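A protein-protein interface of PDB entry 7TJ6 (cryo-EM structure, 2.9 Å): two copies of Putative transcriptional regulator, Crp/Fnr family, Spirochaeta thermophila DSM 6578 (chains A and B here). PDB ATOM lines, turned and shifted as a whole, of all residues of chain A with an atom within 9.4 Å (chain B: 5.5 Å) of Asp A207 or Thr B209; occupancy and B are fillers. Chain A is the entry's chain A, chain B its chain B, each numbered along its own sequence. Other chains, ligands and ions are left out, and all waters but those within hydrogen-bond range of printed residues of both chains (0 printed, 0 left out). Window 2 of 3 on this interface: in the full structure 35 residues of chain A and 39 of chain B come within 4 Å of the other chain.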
ATOM      1  N   TRP A 174      -9.216  -0.765  27.843  1.00  0.00           N
ATOM      2  CA  TRP A 174      -8.834  -1.731  26.818  1.00  0.00           C
ATOM      3  C   TRP A 174      -8.525  -3.103  27.404  1.00  0.00           C
ATOM      4  O   TRP A 174      -8.709  -4.116  26.723  1.00  0.00           O
ATOM      5  CB  TRP A 174      -7.616  -1.216  26.054  1.00  0.00           C
ATOM      6  CG  TRP A 174      -7.053  -2.176  25.050  1.00  0.00           C
ATOM      7  CD1 TRP A 174      -5.926  -2.930  25.185  1.00  0.00           C
ATOM      8  CD2 TRP A 174      -7.564  -2.453  23.741  1.00  0.00           C
ATOM      9  NE1 TRP A 174      -5.715  -3.674  24.054  1.00  0.00           N
ATOM     10  CE2 TRP A 174      -6.706  -3.397  23.150  1.00  0.00           C
ATOM     11  CE3 TRP A 174      -8.668  -1.999  23.016  1.00  0.00           C
ATOM     12  CZ2 TRP A 174      -6.916  -3.894  21.872  1.00  0.00           C
ATOM     13  CZ3 TRP A 174      -8.874  -2.496  21.748  1.00  0.00           C
ATOM     14  CH2 TRP A 174      -8.004  -3.433  21.188  1.00  0.00           C
ATOM     15  N   GLN A 178     -10.503  -7.471  26.513  1.00  0.00           N
ATOM     16  CA  GLN A 178      -9.734  -8.612  26.053  1.00  0.00           C
ATOM     17  C   GLN A 178     -10.320  -9.916  26.590  1.00  0.00           C
ATOM     18  O   GLN A 178     -10.902  -9.947  27.678  1.00  0.00           O
ATOM     19  CB  GLN A 178      -8.273  -8.483  26.468  1.00  0.00           C
ATOM     20  CG  GLN A 178      -7.651  -7.170  26.068  1.00  0.00           C
ATOM     21  CD  GLN A 178      -7.081  -7.223  24.666  1.00  0.00           C
ATOM     22  OE1 GLN A 178      -7.722  -6.798  23.706  1.00  0.00           O
ATOM     23  NE2 GLN A 178      -5.877  -7.761  24.540  1.00  0.00           N
ATOM     24  N   SER A 191       1.233  -4.226  27.896  1.00  0.00           N
ATOM     25  CA  SER A 191       0.741  -4.325  26.526  1.00  0.00           C
ATOM     26  C   SER A 191      -0.408  -3.355  26.273  1.00  0.00           C
ATOM     27  O   SER A 191      -0.464  -2.703  25.221  1.00  0.00           O
ATOM     28  CB  SER A 191       0.302  -5.757  26.232  1.00  0.00           C
ATOM     29  OG  SER A 191      -0.266  -5.855  24.942  1.00  0.00           O
ATOM     30  N   TYR A 194       0.956   0.179  26.067  1.00  0.00           N
ATOM     31  CA  TYR A 194       1.660   0.327  24.799  1.00  0.00           C
ATOM     32  C   TYR A 194       0.689   0.558  23.650  1.00  0.00           C
ATOM     33  O   TYR A 194       0.889   1.462  22.827  1.00  0.00           O
ATOM     34  CB  TYR A 194       2.522  -0.915  24.580  1.00  0.00           C
ATOM     35  CG  TYR A 194       3.082  -1.114  23.201  1.00  0.00           C
ATOM     36  CD1 TYR A 194       3.947  -0.191  22.637  1.00  0.00           C
ATOM     37  CD2 TYR A 194       2.790  -2.260  22.486  1.00  0.00           C
ATOM     38  CE1 TYR A 194       4.473  -0.392  21.386  1.00  0.00           C
ATOM     39  CE2 TYR A 194       3.310  -2.468  21.241  1.00  0.00           C
ATOM     40  CZ  TYR A 194       4.149  -1.534  20.693  1.00  0.00           C
ATOM     41  OH  TYR A 194       4.664  -1.756  19.442  1.00  0.00           O
ATOM     42  N   TRP A 195      -0.406  -0.202  23.620  1.00  0.00           N
ATOM     43  CA  TRP A 195      -1.419   0.008  22.590  1.00  0.00           C
ATOM     44  C   TRP A 195      -2.078   1.374  22.726  1.00  0.00           C
ATOM     45  O   TRP A 195      -2.346   2.046  21.723  1.00  0.00           O
ATOM     46  CB  TRP A 195      -2.483  -1.085  22.656  1.00  0.00           C
ATOM     47  CG  TRP A 195      -3.602  -0.854  21.693  1.00  0.00           C
ATOM     48  CD1 TRP A 195      -3.673  -1.278  20.406  1.00  0.00           C
ATOM     49  CD2 TRP A 195      -4.820  -0.141  21.947  1.00  0.00           C
ATOM     50  NE1 TRP A 195      -4.853  -0.872  19.836  1.00  0.00           N
ATOM     51  CE2 TRP A 195      -5.575  -0.171  20.764  1.00  0.00           C
ATOM     52  CE3 TRP A 195      -5.341   0.523  23.061  1.00  0.00           C
ATOM     53  CZ2 TRP A 195      -6.822   0.434  20.662  1.00  0.00           C
ATOM     54  CZ3 TRP A 195      -6.577   1.123  22.957  1.00  0.00           C
ATOM     55  CH2 TRP A 195      -7.304   1.075  21.768  1.00  0.00           C
ATOM     56  N   THR A 196      -2.355   1.793  23.959  1.00  0.00           N
ATOM     57  CA  THR A 196      -2.989   3.087  24.174  1.00  0.00           C
ATOM     58  C   THR A 196      -2.103   4.238  23.720  1.00  0.00           C
ATOM     59  O   THR A 196      -2.582   5.169  23.065  1.00  0.00           O
ATOM     60  CB  THR A 196      -3.339   3.220  25.652  1.00  0.00           C
ATOM     61  OG1 THR A 196      -4.182   2.129  26.027  1.00  0.00           O
ATOM     62  CG2 THR A 196      -4.066   4.501  25.914  1.00  0.00           C
ATOM     63  N   THR A 198       0.220   4.037  21.486  1.00  0.00           N
ATOM     64  CA  THR A 198       0.381   3.936  20.042  1.00  0.00           C
ATOM     65  C   THR A 198      -0.806   4.568  19.335  1.00  0.00           C
ATOM     66  O   THR A 198      -0.638   5.335  18.381  1.00  0.00           O
ATOM     67  CB  THR A 198       0.549   2.475  19.637  1.00  0.00           C
ATOM     68  OG1 THR A 198       1.617   1.894  20.390  1.00  0.00           O
ATOM     69  CG2 THR A 198       0.884   2.372  18.179  1.00  0.00           C
ATOM     70  N   THR A 199      -2.018   4.236  19.776  1.00  0.00           N
ATOM     71  CA  THR A 199      -3.209   4.821  19.173  1.00  0.00           C
ATOM     72  C   THR A 199      -3.288   6.324  19.432  1.00  0.00           C
ATOM     73  O   THR A 199      -3.532   7.102  18.505  1.00  0.00           O
ATOM     74  CB  THR A 199      -4.459   4.120  19.685  1.00  0.00           C
ATOM     75  OG1 THR A 199      -4.365   2.723  19.392  1.00  0.00           O
ATOM     76  CG2 THR A 199      -5.676   4.669  18.984  1.00  0.00           C
ATOM     77  N   ILE A 203       0.580   6.915  15.785  1.00  0.00           N
ATOM     78  CA  ILE A 203       1.725   6.220  15.221  1.00  0.00           C
ATOM     79  C   ILE A 203       1.314   4.876  14.638  1.00  0.00           C
ATOM     80  O   ILE A 203       1.759   4.507  13.552  1.00  0.00           O
ATOM     81  CB  ILE A 203       2.839   6.075  16.279  1.00  0.00           C
ATOM     82  CG1 ILE A 203       3.393   7.455  16.617  1.00  0.00           C
ATOM     83  CG2 ILE A 203       3.945   5.188  15.790  1.00  0.00           C
ATOM     84  CD1 ILE A 203       4.299   7.493  17.790  1.00  0.00           C
ATOM     85  N   GLY A 204       0.420   4.170  15.320  1.00  0.00           N
ATOM     86  CA  GLY A 204      -0.181   2.966  14.789  1.00  0.00           C
ATOM     87  C   GLY A 204       0.665   1.851  14.218  1.00  0.00           C
ATOM     88  O   GLY A 204       0.547   1.564  13.024  1.00  0.00           O
ATOM     89  N   TYR A 205       1.552   1.255  15.019  1.00  0.00           N
ATOM     90  CA  TYR A 205       2.440   0.220  14.494  1.00  0.00           C
ATOM     91  C   TYR A 205       1.650  -0.927  13.878  1.00  0.00           C
ATOM     92  O   TYR A 205       1.994  -1.417  12.798  1.00  0.00           O
ATOM     93  CB  TYR A 205       3.344  -0.323  15.598  1.00  0.00           C
ATOM     94  CG  TYR A 205       4.484   0.564  16.018  1.00  0.00           C
ATOM     95  CD1 TYR A 205       4.975   1.548  15.182  1.00  0.00           C
ATOM     96  CD2 TYR A 205       5.076   0.409  17.257  1.00  0.00           C
ATOM     97  CE1 TYR A 205       6.022   2.347  15.568  1.00  0.00           C
ATOM     98  CE2 TYR A 205       6.119   1.203  17.651  1.00  0.00           C
ATOM     99  CZ  TYR A 205       6.587   2.172  16.806  1.00  0.00           C
ATOM    100  OH  TYR A 205       7.633   2.965  17.200  1.00  0.00           O
ATOM    101  N   GLY A 206       0.580  -1.358  14.540  1.00  0.00           N
ATOM    102  CA  GLY A 206      -0.300  -2.368  13.989  1.00  0.00           C
ATOM    103  C   GLY A 206      -0.181  -3.727  14.633  1.00  0.00           C
ATOM    104  O   GLY A 206      -0.911  -4.645  14.243  1.00  0.00           O
ATOM    105  N   ASP A 207       0.719  -3.890  15.601  1.00  0.00           N
ATOM    106  CA  ASP A 207       0.934  -5.196  16.213  1.00  0.00           C
ATOM    107  C   ASP A 207      -0.222  -5.586  17.130  1.00  0.00           C
ATOM    108  O   ASP A 207      -0.596  -6.762  17.194  1.00  0.00           O
ATOM    109  CB  ASP A 207       2.277  -5.209  16.942  1.00  0.00           C
ATOM    110  CG  ASP A 207       2.455  -4.025  17.858  1.00  0.00           C
ATOM    111  OD1 ASP A 207       1.520  -3.208  17.971  1.00  0.00           O
ATOM    112  OD2 ASP A 207       3.546  -3.900  18.450  1.00  0.00           O
ATOM    113  N   ILE A 208      -0.797  -4.627  17.849  1.00  0.00           N
ATOM    114  CA  ILE A 208      -1.954  -4.870  18.704  1.00  0.00           C
ATOM    115  C   ILE A 208      -3.164  -4.223  18.046  1.00  0.00           C
ATOM    116  O   ILE A 208      -3.252  -2.994  17.954  1.00  0.00           O
ATOM    117  CB  ILE A 208      -1.738  -4.328  20.121  1.00  0.00           C
ATOM    118  CG1 ILE A 208      -0.358  -4.730  20.632  1.00  0.00           C
ATOM    119  CG2 ILE A 208      -2.827  -4.826  21.050  1.00  0.00           C
ATOM    120  CD1 ILE A 208      -0.098  -4.318  22.051  1.00  0.00           C
ATOM    121  N   THR A 209      -4.088  -5.051  17.568  1.00  0.00           N
ATOM    122  CA  THR A 209      -5.280  -4.616  16.860  1.00  0.00           C
ATOM    123  C   THR A 209      -6.523  -5.280  17.434  1.00  0.00           C
ATOM    124  O   THR A 209      -6.442  -6.378  17.993  1.00  0.00           O
ATOM    125  CB  THR A 209      -5.171  -4.939  15.364  1.00  0.00           C
ATOM    126  OG1 THR A 209      -4.791  -6.310  15.196  1.00  0.00           O
ATOM    127  CG2 THR A 209      -4.146  -4.043  14.701  1.00  0.00           C
ATOM    128  N   PRO A 210      -7.680  -4.627  17.334  1.00  0.00           N
ATOM    129  CA  PRO A 210      -8.918  -5.237  17.828  1.00  0.00           C
ATOM    130  C   PRO A 210      -9.298  -6.476  17.031  1.00  0.00           C
ATOM    131  O   PRO A 210      -9.046  -6.571  15.828  1.00  0.00           O
ATOM    132  CB  PRO A 210      -9.955  -4.126  17.639  1.00  0.00           C
ATOM    133  CG  PRO A 210      -9.381  -3.252  16.588  1.00  0.00           C
ATOM    134  CD  PRO A 210      -7.913  -3.263  16.835  1.00  0.00           C
ATOM    135  N   SER A 211      -9.915  -7.439  17.719  1.00  0.00           N
ATOM    136  CA  SER A 211     -10.406  -8.654  17.079  1.00  0.00           C
ATOM    137  C   SER A 211     -11.923  -8.787  17.111  1.00  0.00           C
ATOM    138  O   SER A 211     -12.550  -8.956  16.061  1.00  0.00           O
ATOM    139  CB  SER A 211      -9.770  -9.880  17.747  1.00  0.00           C
ATOM    140  OG  SER A 211      -8.358  -9.768  17.777  1.00  0.00           O
ATOM    141  N   TRP B 174      18.146   2.641  21.274  1.00  0.00           N
ATOM    142  CA  TRP B 174      17.389   1.482  20.812  1.00  0.00           C
ATOM    143  C   TRP B 174      18.292   0.310  20.447  1.00  0.00           C
ATOM    144  O   TRP B 174      17.871  -0.845  20.557  1.00  0.00           O
ATOM    145  CB  TRP B 174      16.543   1.870  19.602  1.00  0.00           C
ATOM    146  CG  TRP B 174      15.807   0.733  18.959  1.00  0.00           C
ATOM    147  CD1 TRP B 174      16.136   0.100  17.799  1.00  0.00           C
ATOM    148  CD2 TRP B 174      14.595   0.122  19.416  1.00  0.00           C
ATOM    149  NE1 TRP B 174      15.220  -0.879  17.515  1.00  0.00           N
ATOM    150  CE2 TRP B 174      14.261  -0.884  18.492  1.00  0.00           C
ATOM    151  CE3 TRP B 174      13.765   0.325  20.521  1.00  0.00           C
ATOM    152  CZ2 TRP B 174      13.136  -1.683  18.639  1.00  0.00           C
ATOM    153  CZ3 TRP B 174      12.650  -0.472  20.664  1.00  0.00           C
ATOM    154  CH2 TRP B 174      12.345  -1.463  19.729  1.00  0.00           C
ATOM    155  N   TRP B 195      14.048   2.695  12.389  1.00  0.00           N
ATOM    156  CA  TRP B 195      12.983   2.593  13.380  1.00  0.00           C
ATOM    157  C   TRP B 195      12.776   3.911  14.114  1.00  0.00           C
ATOM    158  O   TRP B 195      11.637   4.307  14.390  1.00  0.00           O
ATOM    159  CB  TRP B 195      13.292   1.487  14.386  1.00  0.00           C
ATOM    160  CG  TRP B 195      12.284   1.415  15.487  1.00  0.00           C
ATOM    161  CD1 TRP B 195      11.136   0.693  15.498  1.00  0.00           C
ATOM    162  CD2 TRP B 195      12.341   2.096  16.748  1.00  0.00           C
ATOM    163  NE1 TRP B 195      10.467   0.882  16.682  1.00  0.00           N
ATOM    164  CE2 TRP B 195      11.188   1.740  17.467  1.00  0.00           C
ATOM    165  CE3 TRP B 195      13.255   2.974  17.336  1.00  0.00           C
ATOM    166  CZ2 TRP B 195      10.925   2.229  18.741  1.00  0.00           C
ATOM    167  CZ3 TRP B 195      12.990   3.459  18.599  1.00  0.00           C
ATOM    168  CH2 TRP B 195      11.837   3.086  19.287  1.00  0.00           C
ATOM    169  N   GLY B 206       5.526  -0.535  11.079  1.00  0.00           N
ATOM    170  CA  GLY B 206       5.220  -1.697  11.888  1.00  0.00           C
ATOM    171  C   GLY B 206       6.174  -2.854  11.715  1.00  0.00           C
ATOM    172  O   GLY B 206       6.004  -3.879  12.383  1.00  0.00           O
ATOM    173  N   ASP B 207       7.166  -2.728  10.836  1.00  0.00           N
ATOM    174  CA  ASP B 207       8.077  -3.834  10.570  1.00  0.00           C
ATOM    175  C   ASP B 207       9.043  -4.062  11.729  1.00  0.00           C
ATOM    176  O   ASP B 207       9.381  -5.209  12.042  1.00  0.00           O
ATOM    177  CB  ASP B 207       8.809  -3.595   9.250  1.00  0.00           C
ATOM    178  CG  ASP B 207       9.417  -2.219   9.161  1.00  0.00           C
ATOM    179  OD1 ASP B 207       9.316  -1.454  10.143  1.00  0.00           O
ATOM    180  OD2 ASP B 207       9.978  -1.891   8.096  1.00  0.00           O
ATOM    181  N   ILE B 208       9.501  -2.995  12.375  1.00  0.00           N
ATOM    182  CA  ILE B 208      10.373  -3.094  13.542  1.00  0.00           C
ATOM    183  C   ILE B 208       9.559  -2.695  14.765  1.00  0.00           C
ATOM    184  O   ILE B 208       9.174  -1.531  14.915  1.00  0.00           O
ATOM    185  CB  ILE B 208      11.620  -2.218  13.397  1.00  0.00           C
ATOM    186  CG1 ILE B 208      12.234  -2.405  12.012  1.00  0.00           C
ATOM    187  CG2 ILE B 208      12.625  -2.543  14.483  1.00  0.00           C
ATOM    188  CD1 ILE B 208      13.517  -1.651  11.817  1.00  0.00           C
ATOM    189  N   THR B 209       9.280  -3.666  15.630  1.00  0.00           N
ATOM    190  CA  THR B 209       8.470  -3.483  16.822  1.00  0.00           C
ATOM    191  C   THR B 209       9.167  -4.062  18.045  1.00  0.00           C
ATOM    192  O   THR B 209       9.975  -4.988  17.921  1.00  0.00           O
ATOM    193  CB  THR B 209       7.096  -4.147  16.653  1.00  0.00           C
ATOM    194  OG1 THR B 209       7.269  -5.494  16.195  1.00  0.00           O
ATOM    195  CG2 THR B 209       6.254  -3.377  15.659  1.00  0.00           C
ATOM    196  N   PRO B 210       8.895  -3.521  19.230  1.00  0.00           N
ATOM    197  CA  PRO B 210       9.502  -4.067  20.449  1.00  0.00           C
ATOM    198  C   PRO B 210       9.020  -5.481  20.738  1.00  0.00           C
ATOM    199  O   PRO B 210       7.879  -5.845  20.447  1.00  0.00           O
ATOM    200  CB  PRO B 210       9.037  -3.096  21.537  1.00  0.00           C
ATOM    201  CG  PRO B 210       7.815  -2.466  20.980  1.00  0.00           C
ATOM    202  CD  PRO B 210       8.080  -2.332  19.521  1.00  0.00           C
ATOM    203  N   SER B 211       9.909  -6.286  21.323  1.00  0.00           N
ATOM    204  CA  SER B 211       9.572  -7.646  21.730  1.00  0.00           C
ATOM    205  C   SER B 211       9.612  -7.856  23.238  1.00  0.00           C
ATOM    206  O   SER B 211       8.624  -8.307  23.824  1.00  0.00           O
ATOM    207  CB  SER B 211      10.524  -8.638  21.048  1.00  0.00           C
ATOM    208  OG  SER B 211      10.548  -8.439  19.647  1.00  0.00           O
ATOM    209  N   GLN B 215      11.998  -3.310  25.867  1.00  0.00           N
ATOM    210  CA  GLN B 215      11.842  -2.617  24.594  1.00  0.00           C
ATOM    211  C   GLN B 215      10.466  -1.984  24.468  1.00  0.00           C
ATOM    212  O   GLN B 215      10.323  -0.919  23.863  1.00  0.00           O
ATOM    213  CB  GLN B 215      12.109  -3.571  23.435  1.00  0.00           C
ATOM    214  CG  GLN B 215      13.532  -4.077  23.379  1.00  0.00           C
ATOM    215  CD  GLN B 215      13.734  -5.122  22.307  1.00  0.00           C
ATOM    216  OE1 GLN B 215      12.859  -5.347  21.475  1.00  0.00           O
ATOM    217  NE2 GLN B 215      14.892  -5.766  22.320  1.00  0.00           N
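Asp A207 touches Thr B209, but with the chains exchanged Thr A209 does not touch Asp B207 (12.0 Å). 8 positions are printed for both chains.
The side-chain hydroxyl of Tyr A194 lies within hydrogen-bond range of the side-chain carboxylate of Asp A207, 2.6 Å away. The indole nitrogen (NE1) of Trp B195 sits close to the backbone carbonyl oxygen (O) of Ile B208, 3.3 Å away. The backbone carbonyl oxygen of Tyr A194 is in hydrogen-bond range of the side-chain hydroxyl of Thr A198 (2.6 Å).
CD of Pro B210 touches OH of Tyr A194, 3.5 Å away. Trp B195 touches Tyr A205 (NE1 to OH, 3.6 Å). CA of Gly B206 touches O of Tyr A205, at 3.4 Å. CG2 of Thr B209 touches OD2 of Asp A207 (3.9 Å).
Asp A207 touches just one residue of chain B: Thr B209. Of chain A, only Asp A207 comes within 4 Å of Thr B209. Pro B210 touches one residue of chain A. Printed residues of chain B within 4 Å of Tyr A205: Trp B195 (3.6 Å) and Gly B206 (3.4 Å). Of the printed residues of chain A, Trp B195 touches Tyr A205 (3.6 Å). Of the printed residues of chain A, Gly B206 touches Tyr A205 (3.4 Å). The nearest printed residue of chain B that does not touch Tyr A205 is Thr B209 (4.2 Å).
Hydrophobic or aromatic side chains of chain B within 4 Å of the printed part of chain A: Trp B195 and Pro B210. Of the 17 printed residues of chain A, 3 touch a printed residue of chain B. Among the printed residues, 4 pairs touch across the chains.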
